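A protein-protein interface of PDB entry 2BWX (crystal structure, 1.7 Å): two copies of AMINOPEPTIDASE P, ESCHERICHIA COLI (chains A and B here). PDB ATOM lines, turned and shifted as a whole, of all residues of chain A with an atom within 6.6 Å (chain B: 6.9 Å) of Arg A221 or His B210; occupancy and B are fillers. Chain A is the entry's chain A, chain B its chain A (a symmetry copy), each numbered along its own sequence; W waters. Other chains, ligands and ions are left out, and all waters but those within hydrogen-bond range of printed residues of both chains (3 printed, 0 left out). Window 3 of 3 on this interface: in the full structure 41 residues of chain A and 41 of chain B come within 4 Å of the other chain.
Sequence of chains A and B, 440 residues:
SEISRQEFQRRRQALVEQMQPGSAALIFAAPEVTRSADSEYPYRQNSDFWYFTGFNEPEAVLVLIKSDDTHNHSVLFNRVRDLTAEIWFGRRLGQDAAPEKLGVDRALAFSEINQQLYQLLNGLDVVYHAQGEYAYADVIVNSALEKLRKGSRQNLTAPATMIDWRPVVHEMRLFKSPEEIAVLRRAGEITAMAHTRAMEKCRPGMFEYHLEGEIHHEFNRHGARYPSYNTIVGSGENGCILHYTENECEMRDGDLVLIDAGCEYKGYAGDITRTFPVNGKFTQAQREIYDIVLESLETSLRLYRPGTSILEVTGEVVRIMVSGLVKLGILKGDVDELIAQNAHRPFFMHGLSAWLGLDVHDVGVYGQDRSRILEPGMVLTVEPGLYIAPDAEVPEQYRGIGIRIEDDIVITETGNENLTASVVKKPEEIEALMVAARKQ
Of the printed residues of chain B, His A217 touches Gly B213 and Glu B214.
Of the printed residues of chain B, Asn A220 touches Tyr B209 (2.9 Å), His B210 (3.7 Å) and Gly B213 (3.5 Å).
Arg A221 touches one residue of chain B.
His A222 touches none of the printed residues of chain B.
Of the printed residues of chain B, Gly A223 touches Tyr B209.
His B210 touches two residues of chain A.
Of the printed residues of chain A, Gly B213 touches His A217 and Asn A220.
Printed residues of chain A within 4 Å of Glu B214: His A217 (2.8 Å).
The nearest residue of chain B that does not touch Arg A221 is Tyr B209 (4.6 Å).
Water W3 lies within hydrogen-bond range of OH of Tyr B209 (2.8 Å), O of Arg A221 (2.8 Å) and NE2 of His B210 (3.3 Å).
Water W2 bridges the backbone carbonyl oxygen of Gly B213 and the backbone NH of His A217.
Water W1 bridges ND2 of Asn A220 (2.9 Å) and OE2 of Glu B212 (3.3 Å).
Among the printed residues, merely in contact across the chains: His A217 with Gly B213 (3.5 Å), Asn A220 with His B210 (3.7 Å), Asn A220 with Gly B213 (3.5 Å) and Gly A223 with Tyr B209 (3.5 Å).
NH1 of Arg A197 is in hydrogen-bond range of ND1 of His A217 (2.9 Å).
The side-chain carboxylate (OE1) of Glu A218 is in salt-bridge range of the guanidinium group (NE) of Arg A221 (2.9 Å).
The side-chain amino group (NZ) of Lys B201 is in salt-bridge range of the side-chain carboxylate (OE1) of Glu B214, 2.8 Å away.
A ring nitrogen (ND1) of His B210 sits at hydrogen-bond distance from the backbone NH of Phe B207 (3.1 Å).
The backbone carbonyl oxygen (O) of Asn B247 sits at hydrogen-bond distance from the backbone NH (N) of Tyr B209 (3.0 Å).
The side-chain carboxylate (OE2) of Glu B214 is in hydrogen-bond range of a ring nitrogen (NE2) of His A217, 2.8 Å away.
ND2 of Asn A220 is in hydrogen-bond range of O of Tyr B209 (2.9 Å).
The backbone carbonyl oxygen (O) of Arg A221 lies within hydrogen-bond range of a ring nitrogen (NE2) of His B210, at 3.0 Å.
Of the 15 printed residues of chain B, 4 touch a printed residue of chain A.
Hydrophobic or aromatic side chains of chain B that line the printed part of chain A: Tyr B209 and His B210.
Of the 11 printed residues of chain A, 4 touch a printed residue of chain B.
Among the printed residues, 7 pairs touch across the chains.
Among the printed residues, no Asp or Glu carboxylate lies within 4 Å of a Lys or Arg side-chain nitrogen of the other chain.
No position is printed for both chains.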
ATOM      1  N   MET A 193      10.738  10.681  17.062  1.00  0.00           N
ATOM      2  CA  MET A 193      11.576  11.866  16.839  1.00  0.00           C
ATOM      3  C   MET A 193      13.048  11.549  17.118  1.00  0.00           C
ATOM      4  O   MET A 193      13.951  12.020  16.411  1.00  0.00           O
ATOM      5  CB  MET A 193      11.105  13.057  17.682  1.00  0.00           C
ATOM      6  CG  MET A 193       9.829  13.699  17.148  1.00  0.00           C
ATOM      7  SD  MET A 193       9.382  15.219  18.016  1.00  0.00           S
ATOM      8  CE  MET A 193       8.675  14.558  19.510  1.00  0.00           C
ATOM      9  N   ARG A 197      16.124  11.628  14.469  1.00  0.00           N
ATOM     10  CA  ARG A 197      17.341  12.331  14.821  1.00  0.00           C
ATOM     11  C   ARG A 197      18.576  11.465  14.650  1.00  0.00           C
ATOM     12  O   ARG A 197      19.579  11.938  14.101  1.00  0.00           O
ATOM     13  CB  ARG A 197      17.237  12.912  16.230  1.00  0.00           C
ATOM     14  CG  ARG A 197      18.512  13.589  16.730  1.00  0.00           C
ATOM     15  CD  ARG A 197      18.251  14.240  18.069  1.00  0.00           C
ATOM     16  NE  ARG A 197      19.474  14.751  18.678  1.00  0.00           N
ATOM     17  CZ  ARG A 197      19.513  15.437  19.821  1.00  0.00           C
ATOM     18  NH1 ARG A 197      18.390  15.735  20.460  1.00  0.00           N
ATOM     19  NH2 ARG A 197      20.687  15.822  20.328  1.00  0.00           N
ATOM     20  N   HIS A 216      18.919   9.747  23.603  1.00  0.00           N
ATOM     21  CA  HIS A 216      18.601  10.062  24.993  1.00  0.00           C
ATOM     22  C   HIS A 216      18.355  11.561  25.195  1.00  0.00           C
ATOM     23  O   HIS A 216      17.493  11.944  26.007  1.00  0.00           O
ATOM     24  CB  HIS A 216      19.696   9.564  25.920  1.00  0.00           C
ATOM     25  CG  HIS A 216      19.799   8.071  25.971  1.00  0.00           C
ATOM     26  ND1 HIS A 216      20.834   7.428  26.612  1.00  0.00           N
ATOM     27  CD2 HIS A 216      19.008   7.101  25.461  1.00  0.00           C
ATOM     28  CE1 HIS A 216      20.663   6.120  26.509  1.00  0.00           C
ATOM     29  NE2 HIS A 216      19.558   5.894  25.828  1.00  0.00           N
ATOM     30  N   HIS A 217      19.096  12.387  24.462  1.00  0.00           N
ATOM     31  CA  HIS A 217      18.916  13.840  24.537  1.00  0.00           C
ATOM     32  C   HIS A 217      17.518  14.213  24.003  1.00  0.00           C
ATOM     33  O   HIS A 217      16.789  15.015  24.616  1.00  0.00           O
ATOM     34  CB  HIS A 217      20.009  14.580  23.781  1.00  0.00           C
ATOM     35  CG  HIS A 217      19.904  16.067  23.900  1.00  0.00           C
ATOM     36  ND1 HIS A 217      19.133  16.818  23.043  1.00  0.00           N
ATOM     37  CD2 HIS A 217      20.424  16.936  24.796  1.00  0.00           C
ATOM     38  CE1 HIS A 217      19.208  18.092  23.390  1.00  0.00           C
ATOM     39  NE2 HIS A 217      19.988  18.192  24.448  1.00  0.00           N
ATOM     40  N   GLU A 218      17.128  13.586  22.905  1.00  0.00           N
ATOM     41  CA  GLU A 218      15.798  13.826  22.326  1.00  0.00           C
ATOM     42  C   GLU A 218      14.679  13.365  23.271  1.00  0.00           C
ATOM     43  O   GLU A 218      13.694  14.085  23.473  1.00  0.00           O
ATOM     44  CB  GLU A 218      15.651  13.152  20.966  1.00  0.00           C
ATOM     45  CG  GLU A 218      14.401  13.614  20.176  1.00  0.00           C
ATOM     46  CD  GLU A 218      14.465  15.058  19.688  1.00  0.00           C
ATOM     47  OE1 GLU A 218      15.563  15.660  19.665  1.00  0.00           O
ATOM     48  OE2 GLU A 218      13.402  15.609  19.303  1.00  0.00           O
ATOM     49  N   PHE A 219      14.825  12.183  23.861  1.00  0.00           N
ATOM     50  CA  PHE A 219      13.876  11.769  24.909  1.00  0.00           C
ATOM     51  C   PHE A 219      13.703  12.842  25.983  1.00  0.00           C
ATOM     52  O   PHE A 219      12.584  13.250  26.322  1.00  0.00           O
ATOM     53  CB  PHE A 219      14.315  10.494  25.633  1.00  0.00           C
ATOM     54  CG  PHE A 219      14.326   9.236  24.792  1.00  0.00           C
ATOM     55  CD1 PHE A 219      13.793   9.170  23.492  1.00  0.00           C
ATOM     56  CD2 PHE A 219      14.877   8.075  25.349  1.00  0.00           C
ATOM     57  CE1 PHE A 219      13.832   7.935  22.764  1.00  0.00           C
ATOM     58  CE2 PHE A 219      14.907   6.881  24.639  1.00  0.00           C
ATOM     59  CZ  PHE A 219      14.362   6.800  23.357  1.00  0.00           C
ATOM     60  N   ASN A 220      14.836  13.254  26.548  1.00  0.00           N
ATOM     61  CA  ASN A 220      14.860  14.228  27.623  1.00  0.00           C
ATOM     62  C   ASN A 220      14.182  15.534  27.250  1.00  0.00           C
ATOM     63  O   ASN A 220      13.438  16.106  28.048  1.00  0.00           O
ATOM     64  CB  ASN A 220      16.311  14.470  28.044  1.00  0.00           C
ATOM     65  CG  ASN A 220      16.451  15.601  29.051  1.00  0.00           C
ATOM     66  OD1 ASN A 220      16.392  16.775  28.683  1.00  0.00           O
ATOM     67  ND2 ASN A 220      16.636  15.246  30.319  1.00  0.00           N
ATOM     68  N   ARG A 221      14.429  16.038  26.045  1.00  0.00           N
ATOM     69  CA  ARG A 221      13.903  17.357  25.746  1.00  0.00           C
ATOM     70  C   ARG A 221      12.367  17.409  25.709  1.00  0.00           C
ATOM     71  O   ARG A 221      11.785  18.453  26.007  1.00  0.00           O
ATOM     72  CB  ARG A 221      14.546  17.956  24.533  1.00  0.00           C
ATOM     73  CG  ARG A 221      14.223  17.401  23.272  1.00  0.00           C
ATOM     74  CD  ARG A 221      15.088  18.169  22.241  1.00  0.00           C
ATOM     75  NE  ARG A 221      14.492  18.070  20.924  1.00  0.00           N
ATOM     76  CZ  ARG A 221      13.620  18.931  20.410  1.00  0.00           C
ATOM     77  NH1 ARG A 221      13.266  20.033  21.060  1.00  0.00           N
ATOM     78  NH2 ARG A 221      13.126  18.691  19.202  1.00  0.00           N
ATOM     79  N   HIS A 222      11.739  16.262  25.445  1.00  0.00           N
ATOM     80  CA  HIS A 222      10.277  16.153  25.441  1.00  0.00           C
ATOM     81  C   HIS A 222       9.707  15.705  26.799  1.00  0.00           C
ATOM     82  O   HIS A 222       8.504  15.467  26.925  1.00  0.00           O
ATOM     83  CB  HIS A 222       9.834  15.216  24.321  1.00  0.00           C
ATOM     84  CG  HIS A 222      10.262  15.692  22.974  1.00  0.00           C
ATOM     85  ND1 HIS A 222       9.790  16.867  22.427  1.00  0.00           N
ATOM     86  CD2 HIS A 222      11.170  15.201  22.097  1.00  0.00           C
ATOM     87  CE1 HIS A 222      10.377  17.065  21.258  1.00  0.00           C
ATOM     88  NE2 HIS A 222      11.220  16.071  21.036  1.00  0.00           N
ATOM     89  N   GLY A 223      10.569  15.598  27.806  1.00  0.00           N
ATOM     90  CA  GLY A 223      10.142  15.235  29.157  1.00  0.00           C
ATOM     91  C   GLY A 223      10.093  13.752  29.462  1.00  0.00           C
ATOM     92  O   GLY A 223       9.485  13.350  30.458  1.00  0.00           O
ATOM     93  N   ALA A 224      10.702  12.928  28.610  1.00  0.00           N
ATOM     94  CA  ALA A 224      10.889  11.505  28.886  1.00  0.00           C
ATOM     95  C   ALA A 224      12.353  11.343  29.345  1.00  0.00           C
ATOM     96  O   ALA A 224      13.255  11.188  28.535  1.00  0.00           O
ATOM     97  CB  ALA A 224      10.582  10.699  27.652  1.00  0.00           C
ATOM     98  N   LYS B 201      23.444  27.070  28.012  1.00  0.00           N
ATOM     99  CA  LYS B 201      22.109  26.689  27.518  1.00  0.00           C
ATOM    100  C   LYS B 201      20.970  27.162  28.394  1.00  0.00           C
ATOM    101  O   LYS B 201      19.838  27.311  27.917  1.00  0.00           O
ATOM    102  CB  LYS B 201      22.029  25.169  27.362  1.00  0.00           C
ATOM    103  CG  LYS B 201      22.958  24.603  26.281  1.00  0.00           C
ATOM    104  CD  LYS B 201      22.579  25.071  24.883  1.00  0.00           C
ATOM    105  CE  LYS B 201      23.537  24.524  23.832  1.00  0.00           C
ATOM    106  NZ  LYS B 201      23.357  23.075  23.581  1.00  0.00           N
ATOM    107  N   GLY B 205      12.377  29.429  32.052  1.00  0.00           N
ATOM    108  CA  GLY B 205      11.300  28.675  31.399  1.00  0.00           C
ATOM    109  C   GLY B 205      11.696  27.265  30.999  1.00  0.00           C
ATOM    110  O   GLY B 205      10.830  26.410  30.785  1.00  0.00           O
ATOM    111  N   MET B 206      12.998  27.008  30.864  1.00  0.00           N
ATOM    112  CA  MET B 206      13.470  25.634  30.705  1.00  0.00           C
ATOM    113  C   MET B 206      13.231  24.861  31.996  1.00  0.00           C
ATOM    114  O   MET B 206      13.232  25.435  33.080  1.00  0.00           O
ATOM    115  CB  MET B 206      14.958  25.614  30.335  1.00  0.00           C
ATOM    116  CG  MET B 206      15.192  26.014  28.866  1.00  0.00           C
ATOM    117  SD  MET B 206      16.956  26.207  28.468  1.00  0.00           S
ATOM    118  CE  MET B 206      17.594  24.745  29.259  1.00  0.00           C
ATOM    119  N   PHE B 207      13.023  23.558  31.872  1.00  0.00           N
ATOM    120  CA  PHE B 207      12.945  22.681  33.030  1.00  0.00           C
ATOM    121  C   PHE B 207      14.338  22.276  33.524  1.00  0.00           C
ATOM    122  O   PHE B 207      15.304  22.198  32.750  1.00  0.00           O
ATOM    123  CB  PHE B 207      12.090  21.449  32.721  1.00  0.00           C
ATOM    124  CG  PHE B 207      10.633  21.747  32.706  1.00  0.00           C
ATOM    125  CD1 PHE B 207      10.037  22.277  31.572  1.00  0.00           C
ATOM    126  CD2 PHE B 207       9.872  21.589  33.856  1.00  0.00           C
ATOM    127  CE1 PHE B 207       8.680  22.599  31.569  1.00  0.00           C
ATOM    128  CE2 PHE B 207       8.526  21.904  33.862  1.00  0.00           C
ATOM    129  CZ  PHE B 207       7.932  22.419  32.720  1.00  0.00           C
ATOM    130  N   GLU B 208      14.420  22.004  34.825  1.00  0.00           N
ATOM    131  CA  GLU B 208      15.667  21.577  35.443  1.00  0.00           C
ATOM    132  C   GLU B 208      16.230  20.378  34.663  1.00  0.00           C
ATOM    133  O   GLU B 208      17.429  20.322  34.385  1.00  0.00           O
ATOM    134  CB  GLU B 208      15.432  21.209  36.912  1.00  0.00           C
ATOM    135  CG  GLU B 208      15.114  22.453  37.796  1.00  0.00           C
ATOM    136  CD  GLU B 208      14.515  22.112  39.149  1.00  0.00           C
ATOM    137  OE1 GLU B 208      13.854  21.046  39.290  1.00  0.00           O
ATOM    138  OE2 GLU B 208      14.684  22.954  40.067  1.00  0.00           O
ATOM    139  N   TYR B 209      15.351  19.449  34.281  1.00  0.00           N
ATOM    140  CA  TYR B 209      15.784  18.244  33.558  1.00  0.00           C
ATOM    141  C   TYR B 209      16.392  18.547  32.180  1.00  0.00           C
ATOM    142  O   TYR B 209      17.194  17.764  31.695  1.00  0.00           O
ATOM    143  CB  TYR B 209      14.666  17.193  33.471  1.00  0.00           C
ATOM    144  CG  TYR B 209      13.447  17.584  32.689  1.00  0.00           C
ATOM    145  CD1 TYR B 209      13.444  17.550  31.295  1.00  0.00           C
ATOM    146  CD2 TYR B 209      12.256  17.920  33.331  1.00  0.00           C
ATOM    147  CE1 TYR B 209      12.313  17.867  30.561  1.00  0.00           C
ATOM    148  CE2 TYR B 209      11.114  18.253  32.598  1.00  0.00           C
ATOM    149  CZ  TYR B 209      11.153  18.222  31.211  1.00  0.00           C
ATOM    150  OH  TYR B 209      10.050  18.534  30.459  1.00  0.00           O
ATOM    151  N   HIS B 210      16.058  19.692  31.577  1.00  0.00           N
ATOM    152  CA  HIS B 210      16.690  20.064  30.317  1.00  0.00           C
ATOM    153  C   HIS B 210      18.193  20.219  30.466  1.00  0.00           C
ATOM    154  O   HIS B 210      18.958  19.823  29.581  1.00  0.00           O
ATOM    155  CB  HIS B 210      16.067  21.317  29.725  1.00  0.00           C
ATOM    156  CG  HIS B 210      14.731  21.065  29.101  1.00  0.00           C
ATOM    157  ND1 HIS B 210      13.653  21.893  29.294  1.00  0.00           N
ATOM    158  CD2 HIS B 210      14.304  20.069  28.289  1.00  0.00           C
ATOM    159  CE1 HIS B 210      12.617  21.426  28.618  1.00  0.00           C
ATOM    160  NE2 HIS B 210      12.986  20.316  28.001  1.00  0.00           N
ATOM    161  N   LEU B 211      18.615  20.792  31.583  1.00  0.00           N
ATOM    162  CA  LEU B 211      20.043  20.946  31.830  1.00  0.00           C
ATOM    163  C   LEU B 211      20.723  19.592  32.064  1.00  0.00           C
ATOM    164  O   LEU B 211      21.832  19.372  31.582  1.00  0.00           O
ATOM    165  CB  LEU B 211      20.290  21.916  32.973  1.00  0.00           C
ATOM    166  CG  LEU B 211      19.785  23.350  32.723  1.00  0.00           C
ATOM    167  CD1 LEU B 211      20.303  24.287  33.794  1.00  0.00           C
ATOM    168  CD2 LEU B 211      20.145  23.879  31.342  1.00  0.00           C
ATOM    169  N   GLU B 212      20.045  18.700  32.787  1.00  0.00           N
ATOM    170  CA  GLU B 212      20.486  17.313  32.893  1.00  0.00           C
ATOM    171  C   GLU B 212      20.724  16.712  31.491  1.00  0.00           C
ATOM    172  O   GLU B 212      21.753  16.065  31.257  1.00  0.00           O
ATOM    173  CB  GLU B 212      19.453  16.511  33.689  1.00  0.00           C
ATOM    174  CG  GLU B 212      19.638  14.995  33.667  1.00  0.00           C
ATOM    175  CD  GLU B 212      18.567  14.285  34.480  1.00  0.00           C
ATOM    176  OE1 GLU B 212      17.989  14.921  35.389  1.00  0.00           O
ATOM    177  OE2 GLU B 212      18.282  13.106  34.189  1.00  0.00           O
ATOM    178  N   GLY B 213      19.764  16.909  30.583  1.00  0.00           N
ATOM    179  CA  GLY B 213      19.870  16.428  29.197  1.00  0.00           C
ATOM    180  C   GLY B 213      21.119  16.931  28.490  1.00  0.00           C
ATOM    181  O   GLY B 213      21.838  16.155  27.855  1.00  0.00           O
ATOM    182  N   GLU B 214      21.376  18.235  28.590  1.00  0.00           N
ATOM    183  CA  GLU B 214      22.557  18.843  27.967  1.00  0.00           C
ATOM    184  C   GLU B 214      23.855  18.233  28.533  1.00  0.00           C
ATOM    185  O   GLU B 214      24.771  17.872  27.798  1.00  0.00           O
ATOM    186  CB  GLU B 214      22.557  20.353  28.226  1.00  0.00           C
ATOM    187  CG  GLU B 214      21.417  21.108  27.580  1.00  0.00           C
ATOM    188  CD  GLU B 214      21.417  21.016  26.051  1.00  0.00           C
ATOM    189  OE1 GLU B 214      22.469  21.246  25.455  1.00  0.00           O
ATOM    190  OE2 GLU B 214      20.347  20.767  25.459  1.00  0.00           O
ATOM    191  N   ILE B 215      23.897  18.094  29.855  1.00  0.00           N
ATOM    192  CA  ILE B 215      25.042  17.524  30.577  1.00  0.00           C
ATOM    193  C   ILE B 215      25.321  16.080  30.137  1.00  0.00           C
ATOM    194  O   ILE B 215      26.448  15.750  29.763  1.00  0.00           O
ATOM    195  CB  ILE B 215      24.822  17.638  32.106  1.00  0.00           C
ATOM    196  CG1 ILE B 215      24.915  19.119  32.499  1.00  0.00           C
ATOM    197  CG2 ILE B 215      25.868  16.822  32.879  1.00  0.00           C
ATOM    198  CD1 ILE B 215      24.464  19.440  33.890  1.00  0.00           C
ATOM    199  N   VAL B 233      19.916  19.007  39.618  1.00  0.00           N
ATOM    200  CA  VAL B 233      19.630  20.330  39.030  1.00  0.00           C
ATOM    201  C   VAL B 233      18.568  21.030  39.885  1.00  0.00           C
ATOM    202  O   VAL B 233      17.354  20.919  39.636  1.00  0.00           O
ATOM    203  CB  VAL B 233      19.212  20.262  37.539  1.00  0.00           C
ATOM    204  CG1 VAL B 233      19.081  21.690  36.965  1.00  0.00           C
ATOM    205  CG2 VAL B 233      20.217  19.480  36.719  1.00  0.00           C
ATOM    206  N   ASN B 247      14.518  17.096  39.582  1.00  0.00           N
ATOM    207  CA  ASN B 247      14.811  17.948  38.404  1.00  0.00           C
ATOM    208  C   ASN B 247      13.568  18.217  37.551  1.00  0.00           C
ATOM    209  O   ASN B 247      13.613  18.206  36.321  1.00  0.00           O
ATOM    210  CB  ASN B 247      15.915  17.297  37.567  1.00  0.00           C
ATOM    211  CG  ASN B 247      17.215  17.106  38.361  1.00  0.00           C
ATOM    212  OD1 ASN B 247      17.334  17.566  39.505  1.00  0.00           O
ATOM    213  ND2 ASN B 247      18.168  16.393  37.771  1.00  0.00           N
ATOM    214  N   MET B 251      12.493  26.396  35.616  1.00  0.00           N
ATOM    215  CA  MET B 251      13.479  27.295  36.198  1.00  0.00           C
ATOM    216  C   MET B 251      13.040  28.741  36.013  1.00  0.00           C
ATOM    217  O   MET B 251      12.755  29.165  34.899  1.00  0.00           O
ATOM    218  CB  MET B 251      14.852  27.073  35.571  1.00  0.00           C
ATOM    219  CG  MET B 251      15.428  25.684  35.849  1.00  0.00           C
ATOM    220  SD  MET B 251      17.099  25.450  35.247  1.00  0.00           S
ATOM    221  CE  MET B 251      16.829  25.524  33.482  1.00  0.00           C
HETATM  222  O   HOH W   1      17.479  12.620  31.071  1.00  0.00           O
HETATM  223  O   HOH W   2      20.709  13.659  27.248  1.00  0.00           O
HETATM  224  O   HOH W   3       9.849  19.320  27.817  1.00  0.00           O
